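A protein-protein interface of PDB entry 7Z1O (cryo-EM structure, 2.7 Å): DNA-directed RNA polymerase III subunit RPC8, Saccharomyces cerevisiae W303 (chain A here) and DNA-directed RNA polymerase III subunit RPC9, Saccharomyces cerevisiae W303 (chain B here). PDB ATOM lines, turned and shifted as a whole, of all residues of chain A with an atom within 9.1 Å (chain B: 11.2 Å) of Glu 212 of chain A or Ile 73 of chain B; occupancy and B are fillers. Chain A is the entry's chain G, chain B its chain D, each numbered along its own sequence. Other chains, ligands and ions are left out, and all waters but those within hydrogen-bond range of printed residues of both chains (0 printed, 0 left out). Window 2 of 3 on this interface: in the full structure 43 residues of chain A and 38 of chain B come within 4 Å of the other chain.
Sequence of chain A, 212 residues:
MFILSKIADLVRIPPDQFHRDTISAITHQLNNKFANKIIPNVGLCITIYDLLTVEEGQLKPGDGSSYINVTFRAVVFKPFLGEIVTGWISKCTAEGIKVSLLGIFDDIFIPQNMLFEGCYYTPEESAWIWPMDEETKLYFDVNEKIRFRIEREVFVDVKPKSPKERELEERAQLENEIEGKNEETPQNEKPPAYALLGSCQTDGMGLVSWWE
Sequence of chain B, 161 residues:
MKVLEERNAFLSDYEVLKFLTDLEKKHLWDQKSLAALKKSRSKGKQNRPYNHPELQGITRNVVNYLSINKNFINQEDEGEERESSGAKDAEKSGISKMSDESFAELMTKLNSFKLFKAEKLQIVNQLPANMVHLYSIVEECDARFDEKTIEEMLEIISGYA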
ATOM      1  N   GLU A 144     -20.164 -18.571 -13.409  1.00  0.00           N
ATOM      2  CA  GLU A 144     -20.719 -18.308 -12.091  1.00  0.00           C
ATOM      3  C   GLU A 144     -20.935 -16.810 -11.910  1.00  0.00           C
ATOM      4  O   GLU A 144     -20.305 -15.982 -12.571  1.00  0.00           O
ATOM      5  CB  GLU A 144     -19.802 -18.857 -10.991  1.00  0.00           C
ATOM      6  CG  GLU A 144     -19.966 -20.346 -10.734  1.00  0.00           C
ATOM      7  CD  GLU A 144     -21.344 -20.700 -10.210  1.00  0.00           C
ATOM      8  OE1 GLU A 144     -21.687 -20.261  -9.092  1.00  0.00           O
ATOM      9  OE2 GLU A 144     -22.082 -21.417 -10.916  1.00  0.00           O
ATOM     10  N   LYS A 145     -21.838 -16.466 -10.993  1.00  0.00           N
ATOM     11  CA  LYS A 145     -22.269 -15.088 -10.782  1.00  0.00           C
ATOM     12  C   LYS A 145     -21.293 -14.396  -9.836  1.00  0.00           C
ATOM     13  O   LYS A 145     -21.211 -14.744  -8.653  1.00  0.00           O
ATOM     14  CB  LYS A 145     -23.689 -15.046 -10.224  1.00  0.00           C
ATOM     15  CG  LYS A 145     -24.752 -15.515 -11.200  1.00  0.00           C
ATOM     16  CD  LYS A 145     -26.123 -15.548 -10.547  1.00  0.00           C
ATOM     17  CE  LYS A 145     -26.645 -14.143 -10.300  1.00  0.00           C
ATOM     18  NZ  LYS A 145     -28.037 -14.150  -9.775  1.00  0.00           N
ATOM     19  N   ARG A 147     -19.675 -10.539  -8.402  1.00  0.00           N
ATOM     20  CA  ARG A 147     -19.942  -9.124  -8.203  1.00  0.00           C
ATOM     21  C   ARG A 147     -18.616  -8.385  -8.103  1.00  0.00           C
ATOM     22  O   ARG A 147     -17.707  -8.814  -7.387  1.00  0.00           O
ATOM     23  CB  ARG A 147     -20.777  -8.888  -6.937  1.00  0.00           C
ATOM     24  CG  ARG A 147     -20.561  -7.534  -6.282  1.00  0.00           C
ATOM     25  CD  ARG A 147     -21.401  -7.385  -5.028  1.00  0.00           C
ATOM     26  NE  ARG A 147     -22.820  -7.263  -5.332  1.00  0.00           N
ATOM     27  CZ  ARG A 147     -23.737  -8.153  -4.977  1.00  0.00           C
ATOM     28  NH1 ARG A 147     -23.415  -9.245  -4.303  1.00  0.00           N
ATOM     29  NH2 ARG A 147     -25.006  -7.943  -5.307  1.00  0.00           N
ATOM     30  N   GLY A 204     -17.803  -8.560   0.198  1.00  0.00           N
ATOM     31  CA  GLY A 204     -19.040  -8.591  -0.545  1.00  0.00           C
ATOM     32  C   GLY A 204     -18.873  -8.794  -2.037  1.00  0.00           C
ATOM     33  O   GLY A 204     -19.831  -9.201  -2.702  1.00  0.00           O
ATOM     34  N   LEU A 207     -18.079 -14.096  -5.615  1.00  0.00           N
ATOM     35  CA  LEU A 207     -19.299 -14.865  -5.824  1.00  0.00           C
ATOM     36  C   LEU A 207     -20.427 -14.334  -4.947  1.00  0.00           C
ATOM     37  O   LEU A 207     -20.236 -14.051  -3.762  1.00  0.00           O
ATOM     38  CB  LEU A 207     -19.052 -16.343  -5.521  1.00  0.00           C
ATOM     39  CG  LEU A 207     -18.642 -17.295  -6.648  1.00  0.00           C
ATOM     40  CD1 LEU A 207     -19.797 -17.499  -7.606  1.00  0.00           C
ATOM     41  CD2 LEU A 207     -17.407 -16.804  -7.389  1.00  0.00           C
ATOM     42  N   VAL A 208     -21.612 -14.191  -5.546  1.00  0.00           N
ATOM     43  CA  VAL A 208     -22.762 -13.681  -4.806  1.00  0.00           C
ATOM     44  C   VAL A 208     -23.253 -14.716  -3.798  1.00  0.00           C
ATOM     45  O   VAL A 208     -23.776 -14.368  -2.731  1.00  0.00           O
ATOM     46  CB  VAL A 208     -23.873 -13.239  -5.785  1.00  0.00           C
ATOM     47  CG1 VAL A 208     -24.395 -14.414  -6.607  1.00  0.00           C
ATOM     48  CG2 VAL A 208     -25.007 -12.534  -5.049  1.00  0.00           C
ATOM     49  N   SER A 209     -23.071 -16.004  -4.105  1.00  0.00           N
ATOM     50  CA  SER A 209     -23.538 -17.052  -3.204  1.00  0.00           C
ATOM     51  C   SER A 209     -22.656 -17.170  -1.967  1.00  0.00           C
ATOM     52  O   SER A 209     -23.081 -17.742  -0.956  1.00  0.00           O
ATOM     53  CB  SER A 209     -23.598 -18.390  -3.941  1.00  0.00           C
ATOM     54  OG  SER A 209     -22.298 -18.862  -4.247  1.00  0.00           O
ATOM     55  N   TRP A 210     -21.425 -16.653  -2.031  1.00  0.00           N
ATOM     56  CA  TRP A 210     -20.529 -16.717  -0.880  1.00  0.00           C
ATOM     57  C   TRP A 210     -21.051 -15.878   0.279  1.00  0.00           C
ATOM     58  O   TRP A 210     -20.947 -16.280   1.444  1.00  0.00           O
ATOM     59  CB  TRP A 210     -19.126 -16.258  -1.275  1.00  0.00           C
ATOM     60  CG  TRP A 210     -18.402 -17.202  -2.178  1.00  0.00           C
ATOM     61  CD1 TRP A 210     -18.862 -18.388  -2.667  1.00  0.00           C
ATOM     62  CD2 TRP A 210     -17.082 -17.033  -2.706  1.00  0.00           C
ATOM     63  NE1 TRP A 210     -17.909 -18.971  -3.467  1.00  0.00           N
ATOM     64  CE2 TRP A 210     -16.807 -18.158  -3.507  1.00  0.00           C
ATOM     65  CE3 TRP A 210     -16.107 -16.039  -2.581  1.00  0.00           C
ATOM     66  CZ2 TRP A 210     -15.599 -18.317  -4.180  1.00  0.00           C
ATOM     67  CZ3 TRP A 210     -14.908 -16.200  -3.248  1.00  0.00           C
ATOM     68  CH2 TRP A 210     -14.663 -17.331  -4.036  1.00  0.00           C
ATOM     69  N   TRP A 211     -21.617 -14.707  -0.018  1.00  0.00           N
ATOM     70  CA  TRP A 211     -22.133 -13.803   1.000  1.00  0.00           C
ATOM     71  C   TRP A 211     -23.633 -13.957   1.218  1.00  0.00           C
ATOM     72  O   TRP A 211     -24.320 -12.967   1.496  1.00  0.00           O
ATOM     73  CB  TRP A 211     -21.791 -12.356   0.641  1.00  0.00           C
ATOM     74  CG  TRP A 211     -20.488 -11.894   1.215  1.00  0.00           C
ATOM     75  CD1 TRP A 211     -20.310 -11.137   2.333  1.00  0.00           C
ATOM     76  CD2 TRP A 211     -19.178 -12.168   0.704  1.00  0.00           C
ATOM     77  NE1 TRP A 211     -18.972 -10.915   2.548  1.00  0.00           N
ATOM     78  CE2 TRP A 211     -18.256 -11.539   1.562  1.00  0.00           C
ATOM     79  CE3 TRP A 211     -18.697 -12.879  -0.398  1.00  0.00           C
ATOM     80  CZ2 TRP A 211     -16.879 -11.602   1.353  1.00  0.00           C
ATOM     81  CZ3 TRP A 211     -17.331 -12.944  -0.601  1.00  0.00           C
ATOM     82  CH2 TRP A 211     -16.438 -12.307   0.269  1.00  0.00           C
ATOM     83  N   GLU A 212     -24.156 -15.174   1.088  1.00  0.00           N
ATOM     84  CA  GLU A 212     -25.566 -15.453   1.335  1.00  0.00           C
ATOM     85  C   GLU A 212     -25.956 -15.167   2.783  1.00  0.00           C
ATOM     86  O   GLU A 212     -25.138 -15.298   3.693  1.00  0.00           O
ATOM     87  CB  GLU A 212     -25.885 -16.910   0.993  1.00  0.00           C
ATOM     88  CG  GLU A 212     -27.284 -17.350   1.388  1.00  0.00           C
ATOM     89  CD  GLU A 212     -27.538 -18.814   1.093  1.00  0.00           C
ATOM     90  OE1 GLU A 212     -26.657 -19.463   0.491  1.00  0.00           O
ATOM     91  OE2 GLU A 212     -28.617 -19.318   1.468  1.00  0.00           O
ATOM     92  N   ILE B  68     -33.335 -10.896 -15.025  1.00  0.00           N
ATOM     93  CA  ILE B  68     -32.980 -11.915 -14.045  1.00  0.00           C
ATOM     94  C   ILE B  68     -32.463 -11.261 -12.770  1.00  0.00           C
ATOM     95  O   ILE B  68     -32.065 -10.088 -12.756  1.00  0.00           O
ATOM     96  CB  ILE B  68     -31.946 -12.892 -14.631  1.00  0.00           C
ATOM     97  CG1 ILE B  68     -30.721 -12.132 -15.135  1.00  0.00           C
ATOM     98  CG2 ILE B  68     -32.566 -13.709 -15.752  1.00  0.00           C
ATOM     99  CD1 ILE B  68     -29.706 -13.015 -15.812  1.00  0.00           C
ATOM    100  N   ASN B  69     -32.458 -12.033 -11.685  1.00  0.00           N
ATOM    101  CA  ASN B  69     -32.138 -11.518 -10.356  1.00  0.00           C
ATOM    102  C   ASN B  69     -30.628 -11.531 -10.154  1.00  0.00           C
ATOM    103  O   ASN B  69     -29.993 -12.587 -10.169  1.00  0.00           O
ATOM    104  CB  ASN B  69     -32.837 -12.342  -9.281  1.00  0.00           C
ATOM    105  CG  ASN B  69     -33.240 -11.510  -8.081  1.00  0.00           C
ATOM    106  OD1 ASN B  69     -32.567 -10.541  -7.731  1.00  0.00           O
ATOM    107  ND2 ASN B  69     -34.342 -11.885  -7.444  1.00  0.00           N
ATOM    108  N   LYS B  70     -30.050 -10.343  -9.964  1.00  0.00           N
ATOM    109  CA  LYS B  70     -28.625 -10.256  -9.663  1.00  0.00           C
ATOM    110  C   LYS B  70     -28.354 -10.555  -8.194  1.00  0.00           C
ATOM    111  O   LYS B  70     -27.280 -11.058  -7.843  1.00  0.00           O
ATOM    112  CB  LYS B  70     -28.086  -8.872 -10.037  1.00  0.00           C
ATOM    113  CG  LYS B  70     -27.683  -8.712 -11.502  1.00  0.00           C
ATOM    114  CD  LYS B  70     -28.879  -8.563 -12.429  1.00  0.00           C
ATOM    115  CE  LYS B  70     -29.572  -7.228 -12.222  1.00  0.00           C
ATOM    116  NZ  LYS B  70     -30.705  -7.041 -13.169  1.00  0.00           N
ATOM    117  N   ASN B  71     -29.313 -10.251  -7.321  1.00  0.00           N
ATOM    118  CA  ASN B  71     -29.156 -10.408  -5.877  1.00  0.00           C
ATOM    119  C   ASN B  71     -30.141 -11.462  -5.391  1.00  0.00           C
ATOM    120  O   ASN B  71     -31.326 -11.168  -5.201  1.00  0.00           O
ATOM    121  CB  ASN B  71     -29.388  -9.081  -5.157  1.00  0.00           C
ATOM    122  CG  ASN B  71     -28.448  -7.995  -5.627  1.00  0.00           C
ATOM    123  OD1 ASN B  71     -27.246  -8.213  -5.760  1.00  0.00           O
ATOM    124  ND2 ASN B  71     -28.993  -6.813  -5.889  1.00  0.00           N
ATOM    125  N   PHE B  72     -29.653 -12.681  -5.178  1.00  0.00           N
ATOM    126  CA  PHE B  72     -30.507 -13.762  -4.705  1.00  0.00           C
ATOM    127  C   PHE B  72     -29.639 -14.830  -4.056  1.00  0.00           C
ATOM    128  O   PHE B  72     -28.408 -14.762  -4.089  1.00  0.00           O
ATOM    129  CB  PHE B  72     -31.341 -14.360  -5.845  1.00  0.00           C
ATOM    130  CG  PHE B  72     -32.658 -14.931  -5.398  1.00  0.00           C
ATOM    131  CD1 PHE B  72     -33.682 -14.096  -4.981  1.00  0.00           C
ATOM    132  CD2 PHE B  72     -32.874 -16.299  -5.399  1.00  0.00           C
ATOM    133  CE1 PHE B  72     -34.895 -14.615  -4.569  1.00  0.00           C
ATOM    134  CE2 PHE B  72     -34.084 -16.825  -4.989  1.00  0.00           C
ATOM    135  CZ  PHE B  72     -35.097 -15.982  -4.573  1.00  0.00           C
ATOM    136  N   ILE B  73     -30.311 -15.811  -3.447  1.00  0.00           N
ATOM    137  CA  ILE B  73     -29.615 -16.952  -2.857  1.00  0.00           C
ATOM    138  C   ILE B  73     -28.898 -17.750  -3.940  1.00  0.00           C
ATOM    139  O   ILE B  73     -27.748 -18.172  -3.763  1.00  0.00           O
ATOM    140  CB  ILE B  73     -30.596 -17.836  -2.056  1.00  0.00           C
ATOM    141  CG1 ILE B  73     -31.213 -17.079  -0.867  1.00  0.00           C
ATOM    142  CG2 ILE B  73     -29.916 -19.109  -1.574  1.00  0.00           C
ATOM    143  CD1 ILE B  73     -32.499 -16.316  -1.167  1.00  0.00           C
ATOM    144  N   ASN B  74     -29.557 -17.957  -5.075  1.00  0.00           N
ATOM    145  CA  ASN B  74     -28.985 -18.706  -6.190  1.00  0.00           C
ATOM    146  C   ASN B  74     -27.778 -17.990  -6.792  1.00  0.00           C
ATOM    147  O   ASN B  74     -26.749 -18.609  -7.062  1.00  0.00           O
ATOM    148  CB  ASN B  74     -30.042 -18.939  -7.270  1.00  0.00           C
ATOM    149  CG  ASN B  74     -31.209 -19.767  -6.775  1.00  0.00           C
ATOM    150  OD1 ASN B  74     -32.346 -19.294  -6.734  1.00  0.00           O
ATOM    151  ND2 ASN B  74     -30.936 -21.009  -6.395  1.00  0.00           N
ATOM    152  N   GLU B  91     -36.804 -15.441  -9.025  1.00  0.00           N
ATOM    153  CA  GLU B  91     -35.949 -15.524 -10.202  1.00  0.00           C
ATOM    154  C   GLU B  91     -35.986 -14.214 -10.985  1.00  0.00           C
ATOM    155  O   GLU B  91     -35.137 -13.962 -11.840  1.00  0.00           O
ATOM    156  CB  GLU B  91     -36.377 -16.694 -11.093  1.00  0.00           C
ATOM    157  CG  GLU B  91     -35.298 -17.191 -12.048  1.00  0.00           C
ATOM    158  CD  GLU B  91     -34.077 -17.740 -11.330  1.00  0.00           C
ATOM    159  OE1 GLU B  91     -34.229 -18.288 -10.218  1.00  0.00           O
ATOM    160  OE2 GLU B  91     -32.963 -17.620 -11.881  1.00  0.00           O
ATOM    161  N   LYS B  92     -36.973 -13.378 -10.680  1.00  0.00           N
ATOM    162  CA  LYS B  92     -37.130 -12.076 -11.309  1.00  0.00           C
ATOM    163  C   LYS B  92     -36.344 -11.025 -10.534  1.00  0.00           C
ATOM    164  O   LYS B  92     -36.059 -11.181  -9.345  1.00  0.00           O
ATOM    165  CB  LYS B  92     -38.609 -11.675 -11.385  1.00  0.00           C
ATOM    166  CG  LYS B  92     -39.521 -12.621 -12.179  1.00  0.00           C
ATOM    167  CD  LYS B  92     -39.313 -12.543 -13.694  1.00  0.00           C
ATOM    168  CE  LYS B  92     -38.411 -13.653 -14.227  1.00  0.00           C
ATOM    169  NZ  LYS B  92     -38.306 -13.619 -15.712  1.00  0.00           N
ATOM    170  N   SER B  93     -36.004  -9.942 -11.228  1.00  0.00           N
ATOM    171  CA  SER B  93     -35.184  -8.884 -10.654  1.00  0.00           C
ATOM    172  C   SER B  93     -35.973  -7.901  -9.800  1.00  0.00           C
ATOM    173  O   SER B  93     -35.363  -7.065  -9.126  1.00  0.00           O
ATOM    174  CB  SER B  93     -34.466  -8.114 -11.766  1.00  0.00           C
ATOM    175  OG  SER B  93     -35.373  -7.726 -12.783  1.00  0.00           O
ATOM    176  N   GLN B 126     -29.880  -2.273  -8.337  1.00  0.00           N
ATOM    177  CA  GLN B 126     -29.559  -3.604  -7.837  1.00  0.00           C
ATOM    178  C   GLN B 126     -30.559  -4.150  -6.826  1.00  0.00           C
ATOM    179  O   GLN B 126     -30.732  -5.374  -6.767  1.00  0.00           O
ATOM    180  CB  GLN B 126     -28.153  -3.610  -7.230  1.00  0.00           C
ATOM    181  CG  GLN B 126     -27.063  -3.531  -8.286  1.00  0.00           C
ATOM    182  CD  GLN B 126     -25.681  -3.353  -7.703  1.00  0.00           C
ATOM    183  OE1 GLN B 126     -25.522  -3.122  -6.506  1.00  0.00           O
ATOM    184  NE2 GLN B 126     -24.668  -3.461  -8.553  1.00  0.00           N
ATOM    185  N   LEU B 127     -31.229  -3.284  -6.051  1.00  0.00           N
ATOM    186  CA  LEU B 127     -32.217  -3.664  -5.039  1.00  0.00           C
ATOM    187  C   LEU B 127     -31.657  -4.689  -4.060  1.00  0.00           C
ATOM    188  O   LEU B 127     -32.009  -5.874  -4.140  1.00  0.00           O
ATOM    189  CB  LEU B 127     -33.489  -4.206  -5.697  1.00  0.00           C
ATOM    190  CG  LEU B 127     -34.445  -3.176  -6.295  1.00  0.00           C
ATOM    191  CD1 LEU B 127     -35.584  -3.869  -7.027  1.00  0.00           C
ATOM    192  CD2 LEU B 127     -34.980  -2.253  -5.213  1.00  0.00           C
ATOM    193  N   PRO B 128     -30.773  -4.285  -3.147  1.00  0.00           N
ATOM    194  CA  PRO B 128     -30.141  -5.258  -2.248  1.00  0.00           C
ATOM    195  C   PRO B 128     -31.133  -5.886  -1.280  1.00  0.00           C
ATOM    196  O   PRO B 128     -32.091  -5.255  -0.831  1.00  0.00           O
ATOM    197  CB  PRO B 128     -29.096  -4.425  -1.495  1.00  0.00           C
ATOM    198  CG  PRO B 128     -28.991  -3.140  -2.240  1.00  0.00           C
ATOM    199  CD  PRO B 128     -30.318  -2.914  -2.873  1.00  0.00           C
ATOM    200  N   ALA B 129     -30.880  -7.154  -0.963  1.00  0.00           N
ATOM    201  CA  ALA B 129     -31.571  -7.845   0.115  1.00  0.00           C
ATOM    202  C   ALA B 129     -30.524  -8.391   1.074  1.00  0.00           C
ATOM    203  O   ALA B 129     -30.773  -8.529   2.276  1.00  0.00           O
ATOM    204  CB  ALA B 129     -32.460  -8.965  -0.425  1.00  0.00           C
ATOM    205  N   ASN B 130     -29.343  -8.696   0.541  1.00  0.00           N
ATOM    206  CA  ASN B 130     -28.208  -9.046   1.377  1.00  0.00           C
ATOM    207  C   ASN B 130     -27.695  -7.809   2.106  1.00  0.00           C
ATOM    208  O   ASN B 130     -27.757  -6.688   1.595  1.00  0.00           O
ATOM    209  CB  ASN B 130     -27.096  -9.662   0.534  1.00  0.00           C
ATOM    210  CG  ASN B 130     -26.052 -10.370   1.371  1.00  0.00           C
ATOM    211  OD1 ASN B 130     -26.178 -10.476   2.592  1.00  0.00           O
ATOM    212  ND2 ASN B 130     -25.010 -10.862   0.715  1.00  0.00           N
ATOM    213  N   MET B 131     -27.191  -8.022   3.321  1.00  0.00           N
ATOM    214  CA  MET B 131     -26.817  -6.893   4.164  1.00  0.00           C
ATOM    215  C   MET B 131     -25.470  -6.331   3.703  1.00  0.00           C
ATOM    216  O   MET B 131     -25.302  -5.113   3.551  1.00  0.00           O
ATOM    217  CB  MET B 131     -26.723  -7.357   5.620  1.00  0.00           C
ATOM    218  CG  MET B 131     -26.237  -6.331   6.641  1.00  0.00           C
ATOM    219  SD  MET B 131     -27.456  -4.982   6.750  1.00  0.00           S
ATOM    220  CE  MET B 131     -26.770  -3.625   5.814  1.00  0.00           C
ATOM    221  N   VAL B 132     -24.515  -7.226   3.426  1.00  0.00           N
ATOM    222  CA  VAL B 132     -23.169  -6.828   3.019  1.00  0.00           C
ATOM    223  C   VAL B 132     -23.200  -6.124   1.668  1.00  0.00           C
ATOM    224  O   VAL B 132     -22.363  -5.259   1.392  1.00  0.00           O
ATOM    225  CB  VAL B 132     -22.244  -8.064   3.006  1.00  0.00           C
ATOM    226  CG1 VAL B 132     -20.812  -7.705   2.589  1.00  0.00           C
ATOM    227  CG2 VAL B 132     -22.264  -8.741   4.369  1.00  0.00           C
ATOM    228  N   HIS B 133     -24.175  -6.451   0.819  1.00  0.00           N
ATOM    229  CA  HIS B 133     -24.345  -5.711  -0.427  1.00  0.00           C
ATOM    230  C   HIS B 133     -24.679  -4.245  -0.157  1.00  0.00           C
ATOM    231  O   HIS B 133     -24.170  -3.347  -0.839  1.00  0.00           O
ATOM    232  CB  HIS B 133     -25.430  -6.373  -1.277  1.00  0.00           C
ATOM    233  CG  HIS B 133     -25.567  -5.790  -2.648  1.00  0.00           C
ATOM    234  ND1 HIS B 133     -26.739  -5.856  -3.368  1.00  0.00           N
ATOM    235  CD2 HIS B 133     -24.680  -5.134  -3.432  1.00  0.00           C
ATOM    236  CE1 HIS B 133     -26.570  -5.264  -4.536  1.00  0.00           C
ATOM    237  NE2 HIS B 133     -25.330  -4.818  -4.601  1.00  0.00           N
ATOM    238  N   TYR B 160     -39.419  -4.033  -2.186  1.00  0.00           N
ATOM    239  CA  TYR B 160     -39.315  -3.546  -3.569  1.00  0.00           C
ATOM    240  C   TYR B 160     -40.276  -2.390  -3.843  1.00  0.00           C
ATOM    241  O   TYR B 160     -40.570  -2.070  -4.997  1.00  0.00           O
ATOM    242  CB  TYR B 160     -39.525  -4.674  -4.586  1.00  0.00           C
ATOM    243  CG  TYR B 160     -38.561  -5.834  -4.457  1.00  0.00           C
ATOM    244  CD1 TYR B 160     -37.280  -5.651  -3.954  1.00  0.00           C
ATOM    245  CD2 TYR B 160     -38.935  -7.115  -4.847  1.00  0.00           C
ATOM    246  CE1 TYR B 160     -36.399  -6.711  -3.838  1.00  0.00           C
ATOM    247  CE2 TYR B 160     -38.062  -8.180  -4.736  1.00  0.00           C
ATOM    248  CZ  TYR B 160     -36.795  -7.972  -4.231  1.00  0.00           C
ATOM    249  OH  TYR B 160     -35.924  -9.032  -4.119  1.00  0.00           O
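Lys 145 of chain A touches Lys 70 of chain B (NZ to O, 3.7 Å). Gly 204 of chain A touches Val 132 of chain B (CA to CG1, 3.7 Å). O of Lys 70 of chain B touches CG2 of Val 208 of chain A, 3.9 Å away. CG1 of Val 132 of chain B touches CD1 of Trp 211 of chain A (3.5 Å). Glu 212 of chain A touches Ile 73 of chain B (OE2 to CG2, 3.3 Å).
The backbone carbonyl oxygen of Ile 68 of chain B sits at hydrogen-bond distance from the side-chain amino group of Lys 70 of chain B (3.4 Å). The backbone carbonyl oxygen (O) of Glu 91 of chain B lies within hydrogen-bond range of the backbone NH (N) of Asn 69 of chain B, at 3.3 Å. ND2 of Asn 71 of chain B sits at hydrogen-bond distance from O of Gln 126 of chain B, at 2.4 Å. OD1 of Asn 71 of chain B lies close to ND1 of His 133 of chain B. A ring nitrogen (NE2) of His 133 of chain B lies within hydrogen-bond range of the side-chain amide oxygen of Gln 126 of chain B (2.6 Å). The backbone carbonyl oxygen of Lys 145 of chain A is in hydrogen-bond range of the backbone NH of Val 208 of chain A (3.2 Å).
O of Asn 69 of chain B sits at hydrogen-bond distance from NZ of Lys 145 of chain A, 2.5 Å away. The backbone carbonyl oxygen (O) of Trp 211 of chain A lies close to the side-chain amide oxygen (OD1) of Asn 130 of chain B (3.3 Å). A ring nitrogen (NE2) of His 133 of chain B sits close to the guanidinium group (NH2) of Arg 147 of chain A (3.2 Å). NH2 of Arg 147 of chain A sits close to OD1 of Asn 71 of chain B, at 2.3 Å.
Of chain B, only Ile 73 comes within 4 Å of Glu 212 of chain A. Ser 209 of chain A touches none of the printed residues of chain B. Phe 72 of chain B touches none of the printed residues of chain A. No residue of chain A comes within 4 Å of Asn 74 of chain B. Of the printed residues of chain A, His 133 of chain B touches Arg 147 (3.2 Å). Printed residues of chain A within 4 Å of Lys 70 of chain B: Lys 145 and Val 208. Printed residues of chain B within 4 Å of Arg 147 of chain A: Asn 71 (2.3 Å) and His 133 (3.2 Å). Of the printed residues of chain B, Lys 145 of chain A touches Asn 69 (2.5 Å) and Lys 70 (3.7 Å). Of the printed residues of chain A, Asn 130 of chain B touches Trp 211. Glu 144 of chain A touches none of the printed residues of chain B. The nearest residue of chain A that does not touch Ile 73 of chain B is Ser 209 of chain A (4.2 Å). The nearest printed residue of chain B that does not touch Trp 211 of chain A is Met 131 of chain B (6.0 Å).
Printed residues of chain A that touch a printed residue of chain B: Lys 145, Arg 147, Gly 204, Val 208, Trp 211 and Glu 212. Hydrophobic or aromatic side chains of chain A that line the printed part of chain B: Val 208 and Trp 211. Along chain A the printed residues that touch a printed residue of chain B span positions 145 to 212. Of the 19 printed residues of chain B, 7 touch a printed residue of chain A. Printed residues of chain B that touch a printed residue of chain A: Asn 69, Lys 70, Asn 71, Ile 73, Asn 130, Val 132 and His 133. Hydrophobic or aromatic side chains of chain B within 4 Å of the printed part of chain A: Ile 73, Val 132 and His 133. Among the printed residues, 9 pairs touch across the chains.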
